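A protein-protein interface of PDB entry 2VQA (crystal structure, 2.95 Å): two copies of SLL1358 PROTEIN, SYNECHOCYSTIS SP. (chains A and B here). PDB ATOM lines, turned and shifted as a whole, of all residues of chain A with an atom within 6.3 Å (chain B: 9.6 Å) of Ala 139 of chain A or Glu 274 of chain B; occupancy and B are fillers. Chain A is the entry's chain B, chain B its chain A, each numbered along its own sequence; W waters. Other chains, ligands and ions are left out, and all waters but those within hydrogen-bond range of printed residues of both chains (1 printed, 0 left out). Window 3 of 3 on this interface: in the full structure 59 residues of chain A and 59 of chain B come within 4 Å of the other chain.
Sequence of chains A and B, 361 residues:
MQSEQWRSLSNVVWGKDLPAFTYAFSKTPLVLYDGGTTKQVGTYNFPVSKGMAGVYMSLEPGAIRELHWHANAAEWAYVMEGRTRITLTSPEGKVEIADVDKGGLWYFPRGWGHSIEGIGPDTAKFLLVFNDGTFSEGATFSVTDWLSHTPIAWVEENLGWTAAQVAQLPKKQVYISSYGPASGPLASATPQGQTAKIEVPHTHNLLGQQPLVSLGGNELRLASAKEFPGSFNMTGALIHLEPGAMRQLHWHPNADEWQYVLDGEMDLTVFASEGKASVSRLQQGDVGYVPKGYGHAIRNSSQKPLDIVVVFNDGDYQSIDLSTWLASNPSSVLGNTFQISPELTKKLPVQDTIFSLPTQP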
ATOM      1  N   TRP A  69     -16.254  34.181 -18.864  1.00  0.00           N
ATOM      2  CA  TRP A  69     -15.659  33.757 -20.147  1.00  0.00           C
ATOM      3  C   TRP A  69     -16.643  32.978 -21.013  1.00  0.00           C
ATOM      4  O   TRP A  69     -17.615  32.418 -20.504  1.00  0.00           O
ATOM      5  CB  TRP A  69     -14.396  32.920 -19.938  1.00  0.00           C
ATOM      6  CG  TRP A  69     -14.614  31.465 -19.613  1.00  0.00           C
ATOM      7  CD1 TRP A  69     -14.652  30.425 -20.490  1.00  0.00           C
ATOM      8  CD2 TRP A  69     -14.786  30.893 -18.314  1.00  0.00           C
ATOM      9  NE1 TRP A  69     -14.853  29.240 -19.821  1.00  0.00           N
ATOM     10  CE2 TRP A  69     -14.935  29.502 -18.484  1.00  0.00           C
ATOM     11  CE3 TRP A  69     -14.844  31.424 -17.024  1.00  0.00           C
ATOM     12  CZ2 TRP A  69     -15.129  28.641 -17.422  1.00  0.00           C
ATOM     13  CZ3 TRP A  69     -15.037  30.559 -15.962  1.00  0.00           C
ATOM     14  CH2 TRP A  69     -15.173  29.185 -16.168  1.00  0.00           C
ATOM     15  N   HIS A  70     -16.394  32.945 -22.318  1.00  0.00           N
ATOM     16  CA  HIS A  70     -17.244  32.175 -23.209  1.00  0.00           C
ATOM     17  C   HIS A  70     -16.459  31.667 -24.416  1.00  0.00           C
ATOM     18  O   HIS A  70     -16.108  32.440 -25.311  1.00  0.00           O
ATOM     19  CB  HIS A  70     -18.499  32.965 -23.626  1.00  0.00           C
ATOM     20  CG  HIS A  70     -18.338  34.453 -23.581  1.00  0.00           C
ATOM     21  ND1 HIS A  70     -17.592  35.151 -24.505  1.00  0.00           N
ATOM     22  CD2 HIS A  70     -18.836  35.379 -22.727  1.00  0.00           C
ATOM     23  CE1 HIS A  70     -17.628  36.441 -24.215  1.00  0.00           C
ATOM     24  NE2 HIS A  70     -18.374  36.608 -23.139  1.00  0.00           N
ATOM     25  N   ASN A  72     -17.402  29.599 -26.720  1.00  0.00           N
ATOM     26  CA  ASN A  72     -18.248  29.438 -27.885  1.00  0.00           C
ATOM     27  C   ASN A  72     -18.306  30.690 -28.791  1.00  0.00           C
ATOM     28  O   ASN A  72     -18.838  30.641 -29.900  1.00  0.00           O
ATOM     29  CB  ASN A  72     -19.665  29.012 -27.437  1.00  0.00           C
ATOM     30  CG  ASN A  72     -20.455  30.170 -26.716  1.00  0.00           C
ATOM     31  OD1 ASN A  72     -20.215  30.479 -25.520  1.00  0.00           O
ATOM     32  ND2 ASN A  72     -21.399  30.802 -27.456  1.00  0.00           N
ATOM     33  N   PHE A 135     -25.409  32.945 -29.261  1.00  0.00           N
ATOM     34  CA  PHE A 135     -24.845  33.376 -27.984  1.00  0.00           C
ATOM     35  C   PHE A 135     -25.900  34.088 -27.175  1.00  0.00           C
ATOM     36  O   PHE A 135     -26.698  34.849 -27.722  1.00  0.00           O
ATOM     37  CB  PHE A 135     -23.673  34.328 -28.187  1.00  0.00           C
ATOM     38  CG  PHE A 135     -23.136  34.900 -26.902  1.00  0.00           C
ATOM     39  CD1 PHE A 135     -22.202  34.193 -26.145  1.00  0.00           C
ATOM     40  CD2 PHE A 135     -23.576  36.135 -26.438  1.00  0.00           C
ATOM     41  CE1 PHE A 135     -21.722  34.718 -24.948  1.00  0.00           C
ATOM     42  CE2 PHE A 135     -23.100  36.654 -25.260  1.00  0.00           C
ATOM     43  CZ  PHE A 135     -22.174  35.951 -24.508  1.00  0.00           C
ATOM     44  N   SER A 136     -25.909  33.838 -25.871  1.00  0.00           N
ATOM     45  CA  SER A 136     -26.848  34.493 -24.971  1.00  0.00           C
ATOM     46  C   SER A 136     -26.140  34.839 -23.682  1.00  0.00           C
ATOM     47  O   SER A 136     -25.411  34.018 -23.134  1.00  0.00           O
ATOM     48  CB  SER A 136     -28.034  33.588 -24.684  1.00  0.00           C
ATOM     49  OG  SER A 136     -28.521  33.824 -23.387  1.00  0.00           O
ATOM     50  N   GLU A 137     -26.356  36.067 -23.210  1.00  0.00           N
ATOM     51  CA  GLU A 137     -25.697  36.579 -22.006  1.00  0.00           C
ATOM     52  C   GLU A 137     -26.044  35.715 -20.789  1.00  0.00           C
ATOM     53  O   GLU A 137     -25.288  35.662 -19.816  1.00  0.00           O
ATOM     54  CB  GLU A 137     -26.051  38.060 -21.778  1.00  0.00           C
ATOM     55  CG  GLU A 137     -25.055  38.833 -20.862  1.00  0.00           C
ATOM     56  CD  GLU A 137     -23.734  39.260 -21.550  1.00  0.00           C
ATOM     57  OE1 GLU A 137     -23.677  39.253 -22.798  1.00  0.00           O
ATOM     58  OE2 GLU A 137     -22.755  39.629 -20.846  1.00  0.00           O
ATOM     59  N   GLY A 138     -27.166  35.001 -20.861  1.00  0.00           N
ATOM     60  CA  GLY A 138     -27.551  34.093 -19.793  1.00  0.00           C
ATOM     61  C   GLY A 138     -26.770  32.792 -19.790  1.00  0.00           C
ATOM     62  O   GLY A 138     -26.902  31.973 -18.877  1.00  0.00           O
ATOM     63  N   ALA A 139     -25.953  32.567 -20.807  1.00  0.00           N
ATOM     64  CA  ALA A 139     -25.213  31.302 -20.864  1.00  0.00           C
ATOM     65  C   ALA A 139     -23.700  31.481 -20.841  1.00  0.00           C
ATOM     66  O   ALA A 139     -22.990  30.664 -21.404  1.00  0.00           O
ATOM     67  CB  ALA A 139     -25.647  30.437 -22.078  1.00  0.00           C
ATOM     68  N   THR A 140     -23.209  32.528 -20.186  1.00  0.00           N
ATOM     69  CA  THR A 140     -21.757  32.690 -20.051  1.00  0.00           C
ATOM     70  C   THR A 140     -21.238  31.875 -18.873  1.00  0.00           C
ATOM     71  O   THR A 140     -22.014  31.274 -18.151  1.00  0.00           O
ATOM     72  CB  THR A 140     -21.325  34.167 -19.885  1.00  0.00           C
ATOM     73  OG1 THR A 140     -21.719  34.645 -18.596  1.00  0.00           O
ATOM     74  CG2 THR A 140     -21.933  35.032 -20.980  1.00  0.00           C
ATOM     75  N   PHE A 141     -19.925  31.844 -18.691  1.00  0.00           N
ATOM     76  CA  PHE A 141     -19.335  31.094 -17.596  1.00  0.00           C
ATOM     77  C   PHE A 141     -18.891  32.062 -16.508  1.00  0.00           C
ATOM     78  O   PHE A 141     -17.898  32.783 -16.664  1.00  0.00           O
ATOM     79  CB  PHE A 141     -18.170  30.231 -18.096  1.00  0.00           C
ATOM     80  CG  PHE A 141     -18.608  28.987 -18.835  1.00  0.00           C
ATOM     81  CD1 PHE A 141     -18.507  27.734 -18.241  1.00  0.00           C
ATOM     82  CD2 PHE A 141     -19.142  29.069 -20.119  1.00  0.00           C
ATOM     83  CE1 PHE A 141     -18.914  26.591 -18.915  1.00  0.00           C
ATOM     84  CE2 PHE A 141     -19.557  27.937 -20.788  1.00  0.00           C
ATOM     85  CZ  PHE A 141     -19.438  26.694 -20.187  1.00  0.00           C
ATOM     86  N   ASP A 145     -20.525  31.809 -10.166  1.00  0.00           N
ATOM     87  CA  ASP A 145     -21.261  30.584 -10.469  1.00  0.00           C
ATOM     88  C   ASP A 145     -20.289  29.391 -10.354  1.00  0.00           C
ATOM     89  O   ASP A 145     -20.589  28.375  -9.714  1.00  0.00           O
ATOM     90  CB  ASP A 145     -21.880  30.685 -11.875  1.00  0.00           C
ATOM     91  CG  ASP A 145     -22.964  29.626 -12.142  1.00  0.00           C
ATOM     92  OD1 ASP A 145     -23.643  29.181 -11.195  1.00  0.00           O
ATOM     93  OD2 ASP A 145     -23.155  29.243 -13.319  1.00  0.00           O
ATOM     94  N   HIS A 149     -20.284  26.268  -7.491  1.00  0.00           N
ATOM     95  CA  HIS A 149     -20.688  24.984  -8.029  1.00  0.00           C
ATOM     96  C   HIS A 149     -19.543  23.987  -8.157  1.00  0.00           C
ATOM     97  O   HIS A 149     -19.545  23.161  -9.072  1.00  0.00           O
ATOM     98  CB  HIS A 149     -21.375  25.176  -9.368  1.00  0.00           C
ATOM     99  CG  HIS A 149     -22.752  25.740  -9.252  1.00  0.00           C
ATOM    100  ND1 HIS A 149     -22.993  27.034  -8.849  1.00  0.00           N
ATOM    101  CD2 HIS A 149     -23.965  25.183  -9.481  1.00  0.00           C
ATOM    102  CE1 HIS A 149     -24.296  27.249  -8.824  1.00  0.00           C
ATOM    103  NE2 HIS A 149     -24.910  26.143  -9.211  1.00  0.00           N
ATOM    104  N   GLN A 173     -24.548  32.429  -9.391  1.00  0.00           N
ATOM    105  CA  GLN A 173     -24.035  33.370 -10.377  1.00  0.00           C
ATOM    106  C   GLN A 173     -24.329  34.818  -9.986  1.00  0.00           C
ATOM    107  O   GLN A 173     -25.485  35.177  -9.866  1.00  0.00           O
ATOM    108  CB  GLN A 173     -24.644  33.081 -11.742  1.00  0.00           C
ATOM    109  CG  GLN A 173     -24.571  34.276 -12.676  1.00  0.00           C
ATOM    110  CD  GLN A 173     -24.398  33.898 -14.144  1.00  0.00           C
ATOM    111  OE1 GLN A 173     -24.808  32.827 -14.554  1.00  0.00           O
ATOM    112  NE2 GLN A 173     -23.784  34.790 -14.937  1.00  0.00           N
ATOM    113  N   SER B  10     -23.671  26.074  -3.255  1.00  0.00           N
ATOM    114  CA  SER B  10     -24.974  26.333  -3.856  1.00  0.00           C
ATOM    115  C   SER B  10     -25.934  25.177  -3.639  1.00  0.00           C
ATOM    116  O   SER B  10     -27.123  25.311  -3.899  1.00  0.00           O
ATOM    117  CB  SER B  10     -24.836  26.621  -5.357  1.00  0.00           C
ATOM    118  OG  SER B  10     -24.288  25.501  -6.040  1.00  0.00           O
ATOM    119  N   VAL B  12     -25.969  22.554  -5.447  1.00  0.00           N
ATOM    120  CA  VAL B  12     -26.431  22.119  -6.760  1.00  0.00           C
ATOM    121  C   VAL B  12     -26.608  20.594  -6.718  1.00  0.00           C
ATOM    122  O   VAL B  12     -25.804  19.889  -6.090  1.00  0.00           O
ATOM    123  CB  VAL B  12     -25.438  22.500  -7.883  1.00  0.00           C
ATOM    124  CG1 VAL B  12     -24.025  21.998  -7.543  1.00  0.00           C
ATOM    125  CG2 VAL B  12     -25.923  21.950  -9.232  1.00  0.00           C
ATOM    126  N   VAL B  13     -27.660  20.086  -7.351  1.00  0.00           N
ATOM    127  CA  VAL B  13     -27.787  18.643  -7.481  1.00  0.00           C
ATOM    128  C   VAL B  13     -26.820  18.229  -8.570  1.00  0.00           C
ATOM    129  O   VAL B  13     -27.057  18.494  -9.760  1.00  0.00           O
ATOM    130  CB  VAL B  13     -29.230  18.206  -7.840  1.00  0.00           C
ATOM    131  CG1 VAL B  13     -29.339  16.678  -7.866  1.00  0.00           C
ATOM    132  CG2 VAL B  13     -30.217  18.808  -6.861  1.00  0.00           C
ATOM    133  N   LYS B  16     -27.489  16.966 -12.368  1.00  0.00           N
ATOM    134  CA  LYS B  16     -28.812  17.372 -12.860  1.00  0.00           C
ATOM    135  C   LYS B  16     -28.739  18.262 -14.118  1.00  0.00           C
ATOM    136  O   LYS B  16     -27.933  19.201 -14.166  1.00  0.00           O
ATOM    137  CB  LYS B  16     -29.635  18.058 -11.779  1.00  0.00           C
ATOM    138  CG  LYS B  16     -30.925  18.630 -12.352  1.00  0.00           C
ATOM    139  CD  LYS B  16     -31.950  18.921 -11.274  1.00  0.00           C
ATOM    140  CE  LYS B  16     -33.168  19.575 -11.880  1.00  0.00           C
ATOM    141  NZ  LYS B  16     -33.647  20.636 -10.963  1.00  0.00           N
ATOM    142  N   ASP B  17     -29.579  17.958 -15.117  1.00  0.00           N
ATOM    143  CA  ASP B  17     -29.591  18.654 -16.422  1.00  0.00           C
ATOM    144  C   ASP B  17     -28.291  18.619 -17.221  1.00  0.00           C
ATOM    145  O   ASP B  17     -28.016  19.543 -17.996  1.00  0.00           O
ATOM    146  CB  ASP B  17     -30.020  20.105 -16.256  1.00  0.00           C
ATOM    147  CG  ASP B  17     -31.420  20.217 -15.744  1.00  0.00           C
ATOM    148  OD1 ASP B  17     -32.313  19.563 -16.337  1.00  0.00           O
ATOM    149  OD2 ASP B  17     -31.627  20.925 -14.734  1.00  0.00           O
ATOM    150  N   LEU B  18     -27.491  17.571 -17.037  1.00  0.00           N
ATOM    151  CA  LEU B  18     -26.208  17.480 -17.734  1.00  0.00           C
ATOM    152  C   LEU B  18     -25.976  16.087 -18.253  1.00  0.00           C
ATOM    153  O   LEU B  18     -26.292  15.135 -17.587  1.00  0.00           O
ATOM    154  CB  LEU B  18     -25.047  17.865 -16.815  1.00  0.00           C
ATOM    155  CG  LEU B  18     -24.862  19.342 -16.454  1.00  0.00           C
ATOM    156  CD1 LEU B  18     -23.673  19.504 -15.515  1.00  0.00           C
ATOM    157  CD2 LEU B  18     -24.704  20.227 -17.699  1.00  0.00           C
ATOM    158  N   PHE B 271     -17.917  22.034 -14.644  1.00  0.00           N
ATOM    159  CA  PHE B 271     -18.847  23.141 -14.566  1.00  0.00           C
ATOM    160  C   PHE B 271     -19.287  23.542 -15.995  1.00  0.00           C
ATOM    161  O   PHE B 271     -18.461  23.997 -16.806  1.00  0.00           O
ATOM    162  CB  PHE B 271     -18.171  24.281 -13.787  1.00  0.00           C
ATOM    163  CG  PHE B 271     -18.914  25.583 -13.818  1.00  0.00           C
ATOM    164  CD1 PHE B 271     -20.172  25.704 -13.249  1.00  0.00           C
ATOM    165  CD2 PHE B 271     -18.342  26.702 -14.392  1.00  0.00           C
ATOM    166  CE1 PHE B 271     -20.857  26.916 -13.275  1.00  0.00           C
ATOM    167  CE2 PHE B 271     -19.017  27.911 -14.419  1.00  0.00           C
ATOM    168  CZ  PHE B 271     -20.281  28.017 -13.863  1.00  0.00           C
ATOM    169  N   ALA B 272     -20.564  23.291 -16.328  1.00  0.00           N
ATOM    170  CA  ALA B 272     -21.178  23.813 -17.564  1.00  0.00           C
ATOM    171  C   ALA B 272     -21.547  25.191 -17.120  1.00  0.00           C
ATOM    172  O   ALA B 272     -21.177  25.566 -16.028  1.00  0.00           O
ATOM    173  CB  ALA B 272     -22.398  23.035 -17.930  1.00  0.00           C
ATOM    174  N   SER B 273     -22.257  25.992 -17.876  1.00  0.00           N
ATOM    175  CA  SER B 273     -22.603  27.250 -17.250  1.00  0.00           C
ATOM    176  C   SER B 273     -23.895  27.069 -16.448  1.00  0.00           C
ATOM    177  O   SER B 273     -24.224  25.957 -16.041  1.00  0.00           O
ATOM    178  CB  SER B 273     -22.765  28.302 -18.312  1.00  0.00           C
ATOM    179  OG  SER B 273     -23.380  27.731 -19.450  1.00  0.00           O
ATOM    180  N   GLU B 274     -24.611  28.166 -16.206  1.00  0.00           N
ATOM    181  CA  GLU B 274     -26.008  28.120 -15.769  1.00  0.00           C
ATOM    182  C   GLU B 274     -26.255  27.289 -14.531  1.00  0.00           C
ATOM    183  O   GLU B 274     -27.231  26.543 -14.462  1.00  0.00           O
ATOM    184  CB  GLU B 274     -26.883  27.588 -16.895  1.00  0.00           C
ATOM    185  CG  GLU B 274     -26.525  28.176 -18.255  1.00  0.00           C
ATOM    186  CD  GLU B 274     -27.342  27.602 -19.400  1.00  0.00           C
ATOM    187  OE1 GLU B 274     -27.419  28.266 -20.453  1.00  0.00           O
ATOM    188  OE2 GLU B 274     -27.907  26.497 -19.247  1.00  0.00           O
ATOM    189  N   GLY B 275     -25.377  27.405 -13.548  1.00  0.00           N
ATOM    190  CA  GLY B 275     -25.579  26.682 -12.302  1.00  0.00           C
ATOM    191  C   GLY B 275     -25.734  25.178 -12.465  1.00  0.00           C
ATOM    192  O   GLY B 275     -26.426  24.541 -11.686  1.00  0.00           O
ATOM    193  N   LYS B 276     -25.092  24.592 -13.469  1.00  0.00           N
ATOM    194  CA  LYS B 276     -25.095  23.147 -13.609  1.00  0.00           C
ATOM    195  C   LYS B 276     -23.678  22.616 -13.437  1.00  0.00           C
ATOM    196  O   LYS B 276     -22.723  23.240 -13.903  1.00  0.00           O
ATOM    197  CB  LYS B 276     -25.657  22.766 -14.967  1.00  0.00           C
ATOM    198  CG  LYS B 276     -27.021  23.359 -15.191  1.00  0.00           C
ATOM    199  CD  LYS B 276     -27.557  23.036 -16.560  1.00  0.00           C
ATOM    200  CE  LYS B 276     -28.650  24.020 -16.919  1.00  0.00           C
ATOM    201  NZ  LYS B 276     -28.934  23.940 -18.356  1.00  0.00           N
ATOM    202  N   ALA B 277     -23.528  21.481 -12.761  1.00  0.00           N
ATOM    203  CA  ALA B 277     -22.201  20.944 -12.501  1.00  0.00           C
ATOM    204  C   ALA B 277     -22.264  19.493 -12.054  1.00  0.00           C
ATOM    205  O   ALA B 277     -23.291  19.030 -11.555  1.00  0.00           O
ATOM    206  CB  ALA B 277     -21.499  21.777 -11.466  1.00  0.00           C
ATOM    207  N   GLY B 293     -14.088  24.723 -23.076  1.00  0.00           N
ATOM    208  CA  GLY B 293     -14.548  25.867 -22.313  1.00  0.00           C
ATOM    209  C   GLY B 293     -15.139  25.566 -20.952  1.00  0.00           C
ATOM    210  O   GLY B 293     -15.280  26.470 -20.128  1.00  0.00           O
ATOM    211  N   TYR B 294     -15.510  24.316 -20.702  1.00  0.00           N
ATOM    212  CA  TYR B 294     -16.101  23.981 -19.403  1.00  0.00           C
ATOM    213  C   TYR B 294     -15.046  24.078 -18.322  1.00  0.00           C
ATOM    214  O   TYR B 294     -13.882  23.706 -18.533  1.00  0.00           O
ATOM    215  CB  TYR B 294     -16.721  22.577 -19.391  1.00  0.00           C
ATOM    216  CG  TYR B 294     -18.072  22.420 -20.083  1.00  0.00           C
ATOM    217  CD1 TYR B 294     -18.942  21.397 -19.718  1.00  0.00           C
ATOM    218  CD2 TYR B 294     -18.472  23.284 -21.106  1.00  0.00           C
ATOM    219  CE1 TYR B 294     -20.170  21.234 -20.357  1.00  0.00           C
ATOM    220  CE2 TYR B 294     -19.702  23.134 -21.745  1.00  0.00           C
ATOM    221  CZ  TYR B 294     -20.547  22.108 -21.375  1.00  0.00           C
ATOM    222  OH  TYR B 294     -21.762  21.959 -22.003  1.00  0.00           O
HETATM  223  O   HOH W   1     -17.414  22.142 -11.321  1.00  0.00           O
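N of Glu 274 of chain B lies within hydrogen-bond range of OD2 of Asp 145 of chain A, 3.4 Å away.
O of Gly 293 of chain B lies within hydrogen-bond range of NE1 of Trp 69 of chain A.
The backbone carbonyl oxygen (O) of Gly 275 of chain B lies close to a ring nitrogen (NE2) of His 149 of chain A, 3.3 Å away.
The side-chain carboxylate of Asp 145 of chain A sits at hydrogen-bond distance from the backbone NH of Gly 275 of chain B.
The side-chain hydroxyl (OG) of Ser 10 of chain B sits close to a ring nitrogen (NE2) of His 149 of chain A, at 3.3 Å.
The side-chain carboxylate (OE2) of Glu 274 of chain B is in salt-bridge range of the side-chain amino group (NZ) of Lys 276 of chain B, at 2.9 Å.
The backbone NH (N) of Val 12 of chain B lies close to the side-chain hydroxyl (OG) of Ser 10 of chain B (3.4 Å).
The backbone carbonyl oxygen (O) of Trp 69 of chain A sits at hydrogen-bond distance from the backbone NH (N) of Phe 141 of chain A (3.0 Å).
The side-chain hydroxyl (OG) of Ser 136 of chain A sits close to the backbone NH (N) of Gly 138 of chain A.
ND1 of His 149 of chain A is in hydrogen-bond range of O of Asp 145 of chain A, at 2.9 Å.
Among the printed residues, merely in contact across the chains: Gly 138 of chain A with Glu 274 of chain B, Ala 139 of chain A with Ser 273 of chain B, Ala 139 of chain A with Glu 274 of chain B, Thr 140 of chain A with Ser 273 of chain B, Phe 141 of chain A with Phe 271 of chain B, Phe 141 of chain A with Ala 272 of chain B, Phe 141 of chain A with Ser 273 of chain B, Phe 141 of chain A with Gly 293 of chain B, Phe 141 of chain A with Tyr 294 of chain B, Asp 145 of chain A with Phe 271 of chain B, Asp 145 of chain A with Ser 273 of chain B, His 149 of chain A with Val 12 of chain B and His 149 of chain A with Ala 277 of chain B.
No residue of chain B comes within 4 Å of Ser 136 of chain A.
Of chain B, only Glu 274 (3.9 Å) comes within 4 Å of Gly 138 of chain A.
Thr 140 of chain A touches just one residue of chain B: Ser 273.
Printed residues of chain A within 4 Å of Ser 10 of chain B: His 149 (3.3 Å).
Printed residues of chain B within 4 Å of His 149 of chain A: Ser 10 (3.3 Å), Val 12 (3.5 Å), Gly 275 (3.2 Å) and Ala 277 (3.4 Å).
Printed residues of chain A within 4 Å of Ser 273 of chain B: Ala 139, Thr 140, Phe 141 and Asp 145.
Printed residues of chain A within 4 Å of Gly 275 of chain B: Asp 145 (2.9 Å) and His 149 (3.2 Å).
The nearest printed residue of chain B that does not touch His 149 of chain A is Phe 271 of chain B (4.1 Å).
Of the 13 printed residues of chain A, 7 touch a printed residue of chain B.
Hydrophobic or aromatic side chains of chain B that line the printed part of chain A: Val 12, Phe 271, Ala 277 and Tyr 294.
Among the printed residues, no Asp or Glu carboxylate lies within 4 Å of a Lys or Arg side-chain nitrogen of the other chain.
No position is printed for both chains.
Water W1 lies within hydrogen-bond range of the backbone carbonyl oxygen (O) of His 149 of chain A and the backbone NH (N) of Phe 271 of chain B.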
